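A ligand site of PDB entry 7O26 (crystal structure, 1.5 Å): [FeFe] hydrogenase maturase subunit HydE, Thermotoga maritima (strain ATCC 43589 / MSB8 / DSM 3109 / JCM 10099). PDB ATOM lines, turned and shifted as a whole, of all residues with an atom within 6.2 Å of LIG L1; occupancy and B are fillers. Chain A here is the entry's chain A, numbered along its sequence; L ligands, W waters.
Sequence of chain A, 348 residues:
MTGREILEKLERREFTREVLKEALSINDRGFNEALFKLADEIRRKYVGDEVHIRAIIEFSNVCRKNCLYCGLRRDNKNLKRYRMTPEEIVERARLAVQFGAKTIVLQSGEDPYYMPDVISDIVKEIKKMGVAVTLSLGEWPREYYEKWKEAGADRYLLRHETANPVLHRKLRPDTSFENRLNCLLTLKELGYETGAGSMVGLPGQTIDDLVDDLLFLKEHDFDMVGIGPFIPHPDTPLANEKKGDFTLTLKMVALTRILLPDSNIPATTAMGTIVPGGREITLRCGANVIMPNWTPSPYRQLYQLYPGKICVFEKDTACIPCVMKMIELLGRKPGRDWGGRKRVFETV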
ATOM      1  N   VAL A  62      20.584  -9.983  -6.337  1.00  0.00           N
ATOM      2  CA  VAL A  62      21.869  -9.850  -7.012  1.00  0.00           C
ATOM      3  C   VAL A  62      22.998 -10.207  -6.051  1.00  0.00           C
ATOM      4  O   VAL A  62      23.027  -9.728  -4.908  1.00  0.00           O
ATOM      5  CB  VAL A  62      22.026  -8.419  -7.562  1.00  0.00           C
ATOM      6  CG1 VAL A  62      23.424  -8.208  -8.160  1.00  0.00           C
ATOM      7  CG2 VAL A  62      20.918  -8.136  -8.596  1.00  0.00           C
ATOM      8  N   CYS A  63      23.958 -11.027  -6.511  1.00  0.00           N
ATOM      9  CA  CYS A  63      25.126 -11.345  -5.705  1.00  0.00           C
ATOM     10  C   CYS A  63      26.402 -11.431  -6.533  1.00  0.00           C
ATOM     11  O   CYS A  63      26.407 -12.020  -7.618  1.00  0.00           O
ATOM     12  CB  CYS A  63      24.953 -12.638  -4.910  1.00  0.00           C
ATOM     13  SG  CYS A  63      26.182 -12.739  -3.580  1.00  0.00           S
ATOM     14  N   ARG A  64      27.480 -10.845  -5.992  1.00  0.00           N
ATOM     15  CA  ARG A  64      28.821 -10.913  -6.584  1.00  0.00           C
ATOM     16  C   ARG A  64      29.595 -12.175  -6.191  1.00  0.00           C
ATOM     17  O   ARG A  64      30.637 -12.456  -6.819  1.00  0.00           O
ATOM     18  CB  ARG A  64      29.648  -9.703  -6.182  1.00  0.00           C
ATOM     19  CG  ARG A  64      29.985  -9.668  -4.695  1.00  0.00           C
ATOM     20  CD  ARG A  64      30.707  -8.385  -4.288  1.00  0.00           C
ATOM     21  NE  ARG A  64      30.909  -8.350  -2.826  1.00  0.00           N
ATOM     22  CZ  ARG A  64      31.696  -7.495  -2.178  1.00  0.00           C
ATOM     23  NH1 ARG A  64      32.376  -6.556  -2.843  1.00  0.00           N
ATOM     24  NH2 ARG A  64      31.795  -7.581  -0.846  1.00  0.00           N
ATOM     25  N   LYS A  65      29.141 -12.912  -5.173  1.00  0.00           N
ATOM     26  CA  LYS A  65      29.821 -14.108  -4.694  1.00  0.00           C
ATOM     27  C   LYS A  65      29.229 -15.368  -5.327  1.00  0.00           C
ATOM     28  O   LYS A  65      28.180 -15.342  -5.966  1.00  0.00           O
ATOM     29  CB  LYS A  65      29.758 -14.174  -3.168  1.00  0.00           C
ATOM     30  CG  LYS A  65      30.801 -13.265  -2.482  1.00  0.00           C
ATOM     31  CD  LYS A  65      30.859 -13.510  -0.964  1.00  0.00           C
ATOM     32  CE  LYS A  65      32.125 -12.880  -0.361  1.00  0.00           C
ATOM     33  NZ  LYS A  65      32.313 -11.444  -0.679  1.00  0.00           N
ATOM     34  N   ASN A  66      29.930 -16.488  -5.127  1.00  0.00           N
ATOM     35  CA  ASN A  66      29.664 -17.729  -5.839  1.00  0.00           C
ATOM     36  C   ASN A  66      29.600 -18.908  -4.879  1.00  0.00           C
ATOM     37  O   ASN A  66      29.997 -20.027  -5.222  1.00  0.00           O
ATOM     38  CB  ASN A  66      30.703 -17.968  -6.933  1.00  0.00           C
ATOM     39  CG  ASN A  66      30.141 -18.699  -8.140  1.00  0.00           C
ATOM     40  OD1 ASN A  66      28.952 -18.611  -8.441  1.00  0.00           O
ATOM     41  ND2 ASN A  66      31.013 -19.392  -8.877  1.00  0.00           N
ATOM     42  N   CYS A  67      29.087 -18.692  -3.672  1.00  0.00           N
ATOM     43  CA  CYS A  67      29.005 -19.788  -2.691  1.00  0.00           C
ATOM     44  C   CYS A  67      28.325 -21.012  -3.304  1.00  0.00           C
ATOM     45  O   CYS A  67      27.274 -20.904  -3.937  1.00  0.00           O
ATOM     46  CB  CYS A  67      28.220 -19.336  -1.448  1.00  0.00           C
ATOM     47  SG  CYS A  67      28.797 -17.790  -0.719  1.00  0.00           S
ATOM     48  N   TYR A  69      26.674 -23.549  -2.198  1.00  0.00           N
ATOM     49  CA  TYR A  69      25.385 -24.039  -1.731  1.00  0.00           C
ATOM     50  C   TYR A  69      24.213 -23.140  -2.128  1.00  0.00           C
ATOM     51  O   TYR A  69      23.055 -23.581  -2.037  1.00  0.00           O
ATOM     52  CB  TYR A  69      25.395 -24.144  -0.188  1.00  0.00           C
ATOM     53  CG  TYR A  69      26.026 -22.957   0.521  1.00  0.00           C
ATOM     54  CD1 TYR A  69      25.314 -21.788   0.767  1.00  0.00           C
ATOM     55  CD2 TYR A  69      27.370 -23.004   0.935  1.00  0.00           C
ATOM     56  CE1 TYR A  69      25.903 -20.694   1.407  1.00  0.00           C
ATOM     57  CE2 TYR A  69      27.949 -21.922   1.591  1.00  0.00           C
ATOM     58  CZ  TYR A  69      27.221 -20.775   1.807  1.00  0.00           C
ATOM     59  OH  TYR A  69      27.793 -19.699   2.448  1.00  0.00           O
ATOM     60  N   CYS A  70      24.462 -21.898  -2.536  1.00  0.00           N
ATOM     61  CA  CYS A  70      23.432 -20.874  -2.568  1.00  0.00           C
ATOM     62  C   CYS A  70      22.853 -20.688  -3.963  1.00  0.00           C
ATOM     63  O   CYS A  70      23.617 -20.490  -4.930  1.00  0.00           O
ATOM     64  CB  CYS A  70      24.030 -19.555  -2.101  1.00  0.00           C
ATOM     65  SG  CYS A  70      22.824 -18.249  -1.998  1.00  0.00           S
ATOM     66  N   GLY A  71      21.519 -20.686  -4.072  1.00  0.00           N
ATOM     67  CA  GLY A  71      20.863 -20.452  -5.355  1.00  0.00           C
ATOM     68  C   GLY A  71      21.062 -19.045  -5.943  1.00  0.00           C
ATOM     69  O   GLY A  71      20.803 -18.856  -7.137  1.00  0.00           O
ATOM     70  N   LEU A  72      21.468 -18.056  -5.140  1.00  0.00           N
ATOM     71  CA  LEU A  72      21.776 -16.714  -5.655  1.00  0.00           C
ATOM     72  C   LEU A  72      23.226 -16.559  -6.116  1.00  0.00           C
ATOM     73  O   LEU A  72      23.614 -15.468  -6.532  1.00  0.00           O
ATOM     74  CB  LEU A  72      21.483 -15.664  -4.565  1.00  0.00           C
ATOM     75  CG  LEU A  72      20.140 -15.691  -3.841  1.00  0.00           C
ATOM     76  CD1 LEU A  72      19.957 -14.370  -3.062  1.00  0.00           C
ATOM     77  CD2 LEU A  72      18.977 -15.929  -4.791  1.00  0.00           C
ATOM     78  N   ARG A  73      24.038 -17.619  -6.038  1.00  0.00           N
ATOM     79  CA  ARG A  73      25.422 -17.523  -6.488  1.00  0.00           C
ATOM     80  C   ARG A  73      25.512 -16.935  -7.892  1.00  0.00           C
ATOM     81  O   ARG A  73      24.636 -17.157  -8.741  1.00  0.00           O
ATOM     82  CB  ARG A  73      26.106 -18.884  -6.436  1.00  0.00           C
ATOM     83  CG  ARG A  73      25.532 -19.914  -7.401  1.00  0.00           C
ATOM     84  CD  ARG A  73      25.942 -21.320  -7.001  1.00  0.00           C
ATOM     85  NE  ARG A  73      27.385 -21.443  -6.803  1.00  0.00           N
ATOM     86  CZ  ARG A  73      28.251 -21.777  -7.750  1.00  0.00           C
ATOM     87  NH1 ARG A  73      27.838 -22.033  -9.005  1.00  0.00           N
ATOM     88  NH2 ARG A  73      29.536 -21.862  -7.463  1.00  0.00           N
ATOM     89  N   ARG A  74      26.593 -16.188  -8.163  1.00  0.00           N
ATOM     90  CA  ARG A  74      26.632 -15.384  -9.374  1.00  0.00           C
ATOM     91  C   ARG A  74      26.610 -16.225 -10.644  1.00  0.00           C
ATOM     92  O   ARG A  74      26.133 -15.760 -11.689  1.00  0.00           O
ATOM     93  CB  ARG A  74      27.838 -14.440  -9.379  1.00  0.00           C
ATOM     94  CG  ARG A  74      29.175 -15.113  -9.404  1.00  0.00           C
ATOM     95  CD  ARG A  74      30.323 -14.192  -9.861  1.00  0.00           C
ATOM     96  NE  ARG A  74      31.537 -14.991  -9.971  1.00  0.00           N
ATOM     97  CZ  ARG A  74      32.367 -15.283  -8.969  1.00  0.00           C
ATOM     98  NH1 ARG A  74      32.151 -14.810  -7.744  1.00  0.00           N
ATOM     99  NH2 ARG A  74      33.415 -16.058  -9.201  1.00  0.00           N
ATOM    100  N   SER A 108      19.971  -9.238   1.641  1.00  0.00           N
ATOM    101  CA  SER A 108      20.167  -9.305   0.193  1.00  0.00           C
ATOM    102  C   SER A 108      21.366 -10.179  -0.126  1.00  0.00           C
ATOM    103  O   SER A 108      22.167 -10.516   0.751  1.00  0.00           O
ATOM    104  CB  SER A 108      20.395  -7.877  -0.371  1.00  0.00           C
ATOM    105  OG  SER A 108      21.560  -7.321   0.183  1.00  0.00           O
ATOM    106  N   GLY A 109      21.500 -10.534  -1.397  1.00  0.00           N
ATOM    107  CA  GLY A 109      22.798 -10.937  -1.917  1.00  0.00           C
ATOM    108  C   GLY A 109      23.806  -9.816  -1.751  1.00  0.00           C
ATOM    109  O   GLY A 109      23.469  -8.683  -1.436  1.00  0.00           O
ATOM    110  N   GLU A 110      25.083 -10.147  -1.946  1.00  0.00           N
ATOM    111  CA  GLU A 110      26.109  -9.110  -1.911  1.00  0.00           C
ATOM    112  C   GLU A 110      26.011  -8.317  -3.202  1.00  0.00           C
ATOM    113  O   GLU A 110      26.709  -8.579  -4.182  1.00  0.00           O
ATOM    114  CB  GLU A 110      27.514  -9.701  -1.715  1.00  0.00           C
ATOM    115  CG  GLU A 110      27.713 -10.218  -0.291  1.00  0.00           C
ATOM    116  CD  GLU A 110      29.171 -10.451   0.046  1.00  0.00           C
ATOM    117  OE1 GLU A 110      30.059 -10.057  -0.763  1.00  0.00           O
ATOM    118  OE2 GLU A 110      29.425 -11.023   1.129  1.00  0.00           O
ATOM    119  N   GLY A 138      25.971  -9.325   4.006  1.00  0.00           N
ATOM    120  CA  GLY A 138      27.207 -10.016   3.664  1.00  0.00           C
ATOM    121  C   GLY A 138      28.459  -9.298   4.138  1.00  0.00           C
ATOM    122  O   GLY A 138      28.424  -8.516   5.096  1.00  0.00           O
ATOM    123  N   GLU A 161      28.492 -19.847   8.901  1.00  0.00           N
ATOM    124  CA  GLU A 161      28.286 -20.929   7.923  1.00  0.00           C
ATOM    125  C   GLU A 161      28.934 -22.225   8.358  1.00  0.00           C
ATOM    126  O   GLU A 161      28.257 -23.257   8.482  1.00  0.00           O
ATOM    127  CB  GLU A 161      28.733 -20.543   6.490  1.00  0.00           C
ATOM    128  CG  GLU A 161      28.302 -19.119   6.072  1.00  0.00           C
ATOM    129  CD  GLU A 161      26.774 -18.913   5.975  1.00  0.00           C
ATOM    130  OE1 GLU A 161      25.973 -19.759   6.422  1.00  0.00           O
ATOM    131  OE2 GLU A 161      26.372 -17.855   5.428  1.00  0.00           O
ATOM    132  N   ARG A 172      32.949 -21.436  -0.124  1.00  0.00           N
ATOM    133  CA  ARG A 172      32.839 -19.990  -0.329  1.00  0.00           C
ATOM    134  C   ARG A 172      34.140 -19.526  -0.956  1.00  0.00           C
ATOM    135  O   ARG A 172      34.984 -18.901  -0.304  1.00  0.00           O
ATOM    136  CB  ARG A 172      32.555 -19.293   0.996  1.00  0.00           C
ATOM    137  CG  ARG A 172      31.394 -19.994   1.750  1.00  0.00           C
ATOM    138  CD  ARG A 172      30.898 -19.218   2.991  1.00  0.00           C
ATOM    139  NE  ARG A 172      30.299 -17.971   2.540  1.00  0.00           N
ATOM    140  CZ  ARG A 172      30.761 -16.768   2.819  1.00  0.00           C
ATOM    141  NH1 ARG A 172      31.803 -16.628   3.644  1.00  0.00           N
ATOM    142  NH2 ARG A 172      30.164 -15.714   2.287  1.00  0.00           N
ATOM    143  N   ARG A 180      35.444 -13.987   7.327  1.00  0.00           N
ATOM    144  CA  ARG A 180      34.126 -14.014   7.964  1.00  0.00           C
ATOM    145  C   ARG A 180      34.235 -13.683   9.445  1.00  0.00           C
ATOM    146  O   ARG A 180      33.431 -12.917   9.977  1.00  0.00           O
ATOM    147  CB  ARG A 180      33.491 -15.411   7.813  1.00  0.00           C
ATOM    148  CG  ARG A 180      31.951 -15.462   8.016  1.00  0.00           C
ATOM    149  CD  ARG A 180      31.251 -14.908   6.786  1.00  0.00           C
ATOM    150  NE  ARG A 180      29.801 -15.142   6.804  1.00  0.00           N
ATOM    151  CZ  ARG A 180      28.976 -14.724   5.847  1.00  0.00           C
ATOM    152  NH1 ARG A 180      29.472 -14.042   4.798  1.00  0.00           N
ATOM    153  NH2 ARG A 180      27.679 -15.000   5.926  1.00  0.00           N
ATOM    154  N   TYR A 303      13.706 -15.122  -4.594  1.00  0.00           N
ATOM    155  CA  TYR A 303      14.771 -15.149  -3.609  1.00  0.00           C
ATOM    156  C   TYR A 303      14.923 -16.596  -3.148  1.00  0.00           C
ATOM    157  O   TYR A 303      14.458 -16.995  -2.094  1.00  0.00           O
ATOM    158  CB  TYR A 303      14.456 -14.182  -2.493  1.00  0.00           C
ATOM    159  CG  TYR A 303      15.618 -13.816  -1.619  1.00  0.00           C
ATOM    160  CD1 TYR A 303      16.461 -12.766  -1.976  1.00  0.00           C
ATOM    161  CD2 TYR A 303      15.830 -14.470  -0.431  1.00  0.00           C
ATOM    162  CE1 TYR A 303      17.509 -12.400  -1.151  1.00  0.00           C
ATOM    163  CE2 TYR A 303      16.874 -14.104   0.404  1.00  0.00           C
ATOM    164  CZ  TYR A 303      17.710 -13.080   0.020  1.00  0.00           C
ATOM    165  OH  TYR A 303      18.734 -12.700   0.858  1.00  0.00           O
ATOM    166  N   LEU A 305      17.249 -19.044  -2.112  1.00  0.00           N
ATOM    167  CA  LEU A 305      18.486 -19.564  -1.534  1.00  0.00           C
ATOM    168  C   LEU A 305      18.539 -21.087  -1.655  1.00  0.00           C
ATOM    169  O   LEU A 305      19.573 -21.659  -2.018  1.00  0.00           O
ATOM    170  CB  LEU A 305      18.592 -19.147  -0.069  1.00  0.00           C
ATOM    171  CG  LEU A 305      18.574 -17.656   0.249  1.00  0.00           C
ATOM    172  CD1 LEU A 305      18.562 -17.490   1.752  1.00  0.00           C
ATOM    173  CD2 LEU A 305      19.774 -16.967  -0.304  1.00  0.00           C
HETATM  174 FE1  LIG L   1      24.275 -16.613  -1.446  1.00  0.00          FE
HETATM  175 FE2  LIG L   1      25.709 -14.444  -2.207  1.00  0.00          FE
HETATM  176 FE3  LIG L   1      26.896 -16.458  -0.778  1.00  0.00          FE
HETATM  177 FE4  LIG L   1      24.969 -14.746   0.515  1.00  0.00          FE
HETATM  178  S1  LIG L   1      27.058 -14.222  -0.373  1.00  0.00           S
HETATM  179  S2  LIG L   1      25.173 -17.052   0.618  1.00  0.00           S
HETATM  180  S3  LIG L   1      23.587 -14.443  -1.321  1.00  0.00           S
HETATM  181  S4  LIG L   1      26.043 -16.596  -2.907  1.00  0.00           S
HETATM  182  N1  LG2 L   2      24.548 -12.361   1.230  1.00  0.00           N
HETATM  183  C1  LG2 L   2      24.532 -12.289   2.679  1.00  0.00           C
HETATM  184  C2  LG2 L   2      25.349 -13.433   3.297  1.00  0.00           C
HETATM  185  O1  LG2 L   2      25.744 -13.357   4.474  1.00  0.00           O
HETATM  186  C3  LG2 L   2      23.096 -12.322   3.190  1.00  0.00           C
HETATM  187  C4  LG2 L   2      22.573 -13.712   3.402  1.00  0.00           C
HETATM  188  S1  LG2 L   2      22.562 -14.859   1.979  1.00  0.00           S
HETATM  189  C5  LG2 L   2      21.274 -14.089   1.031  1.00  0.00           C
HETATM  190  O2  LG2 L   2      25.637 -14.444   2.634  1.00  0.00           O
HETATM  191  N1  LG3 L   3      20.476 -24.376   2.412  1.00  0.00           N
HETATM  192  C1  LG3 L   3      20.294 -23.904   3.662  1.00  0.00           C
HETATM  193  N2  LG3 L   3      20.639 -22.677   4.002  1.00  0.00           N
HETATM  194  C2  LG3 L   3      21.219 -21.846   3.067  1.00  0.00           C
HETATM  195  N3  LG3 L   3      21.674 -20.584   3.131  1.00  0.00           N
HETATM  196  C3  LG3 L   3      22.164 -20.227   1.931  1.00  0.00           C
HETATM  197  N4  LG3 L   3      22.006 -21.237   1.078  1.00  0.00           N
HETATM  198  C4  LG3 L   3      21.434 -22.279   1.791  1.00  0.00           C
HETATM  199  C5  LG3 L   3      21.025 -23.608   1.458  1.00  0.00           C
HETATM  200  N5  LG3 L   3      21.199 -24.124   0.114  1.00  0.00           N
HETATM  201  C6  LG3 L   3      21.692 -19.842   4.260  1.00  0.00           C
HETATM  202  C7  LG3 L   3      23.133 -19.311   4.634  1.00  0.00           C
HETATM  203  C8  LG3 L   3      23.068 -18.056   4.520  1.00  0.00           C
HETATM  204  C9  LG3 L   3      21.491 -17.779   4.845  1.00  0.00           C
HETATM  205  C10 LG3 L   3      21.090 -16.394   4.435  1.00  0.00           C
HETATM  206  O1  LG3 L   3      20.909 -18.602   4.068  1.00  0.00           O
HETATM  207  O2  LG3 L   3      23.472 -19.800   6.033  1.00  0.00           O
HETATM  208  O3  LG3 L   3      23.912 -17.240   5.440  1.00  0.00           O
HETATM  209  O   HOH W   1      27.297 -16.998   3.040  1.00  0.00           O
HETATM  210  O   HOH W   2      28.367 -13.140   2.402  1.00  0.00           O
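Merely in contact with LIG L1: Gly 109 (3.6 Å), Arg 73 (3.8 Å), Tyr 69 (3.8 Å) and Lys 65 (3.9 Å). Of the 21 residues printed, 7 come within 4 Å of LIG L1. The nearest printed residue that does not touch LIG L1 is Leu 72 (4.03 Å).
The side-chain sulfur (SG) of Cys 63 is bound to an iron atom (FE2) of LIG L1 (2.2 Å). FE1 of LIG L1 is bound by SG of Cys 70. A sulfur (S4) of LIG L1 sits close to the backbone NH (N) of Cys 67. The side-chain sulfur (SG) of Cys 67 binds an iron atom (FE3) of LIG L1 (2.3 Å). The backbone carbonyl oxygen (O) of Ser 108 lies close to a nitrogen (N1) of LG2 L2 (3.1 Å). An oxygen (O1) of LG2 L2 is in salt-bridge range of the guanidinium group of Arg 180 (2.9 Å). O of Tyr 69 sits at hydrogen-bond distance from N5 of LG3 L3 (2.9 Å). O2 of LG3 L3 sits at hydrogen-bond distance from OE1 of Glu 161 (2.5 Å).
An iron atom (FE4) of LIG L1 is bound by an oxygen (O2) of LG2 L2.
Water W1 lies within hydrogen-bond range of the side-chain carboxylate of Glu 161, the side-chain hydroxyl of Tyr 69, the guanidinium group of Arg 172 and a sulfur (S2) of LIG L1. Water W2 lies within hydrogen-bond range of OE2 of Glu 110 (2.7 Å), NH1 of Arg 180 (2.8 Å), NH2 of Arg 172 (3.1 Å), S1 of LIG L1 (3.3 Å) and O1 of LG2 L2 (3.3 Å).
The side-chain sulfur (SG) of Cys 63 lies close to the backbone NH (N) of Lys 65, at 3.4 Å. N of Glu 110 sits close to SG of Cys 63 (3.3 Å). N of Leu 72 lies close to SG of Cys 70, at 3.4 Å. The backbone carbonyl oxygen (O) of Cys 67 lies within hydrogen-bond range of the guanidinium group (NE) of Arg 73 (2.9 Å). The side-chain sulfur (SG) of Cys 67 sits close to the guanidinium group (NE) of Arg 172 (3.6 Å). The guanidinium group (NH2) of Arg 73 sits at hydrogen-bond distance from the backbone carbonyl oxygen (O) of Asn 66. OH of Tyr 69 is in hydrogen-bond range of NE of Arg 172, at 3.0 Å. The backbone carbonyl oxygen (O) of Lys 65 sits at hydrogen-bond distance from the backbone NH (N) of Arg 74 (2.8 Å).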
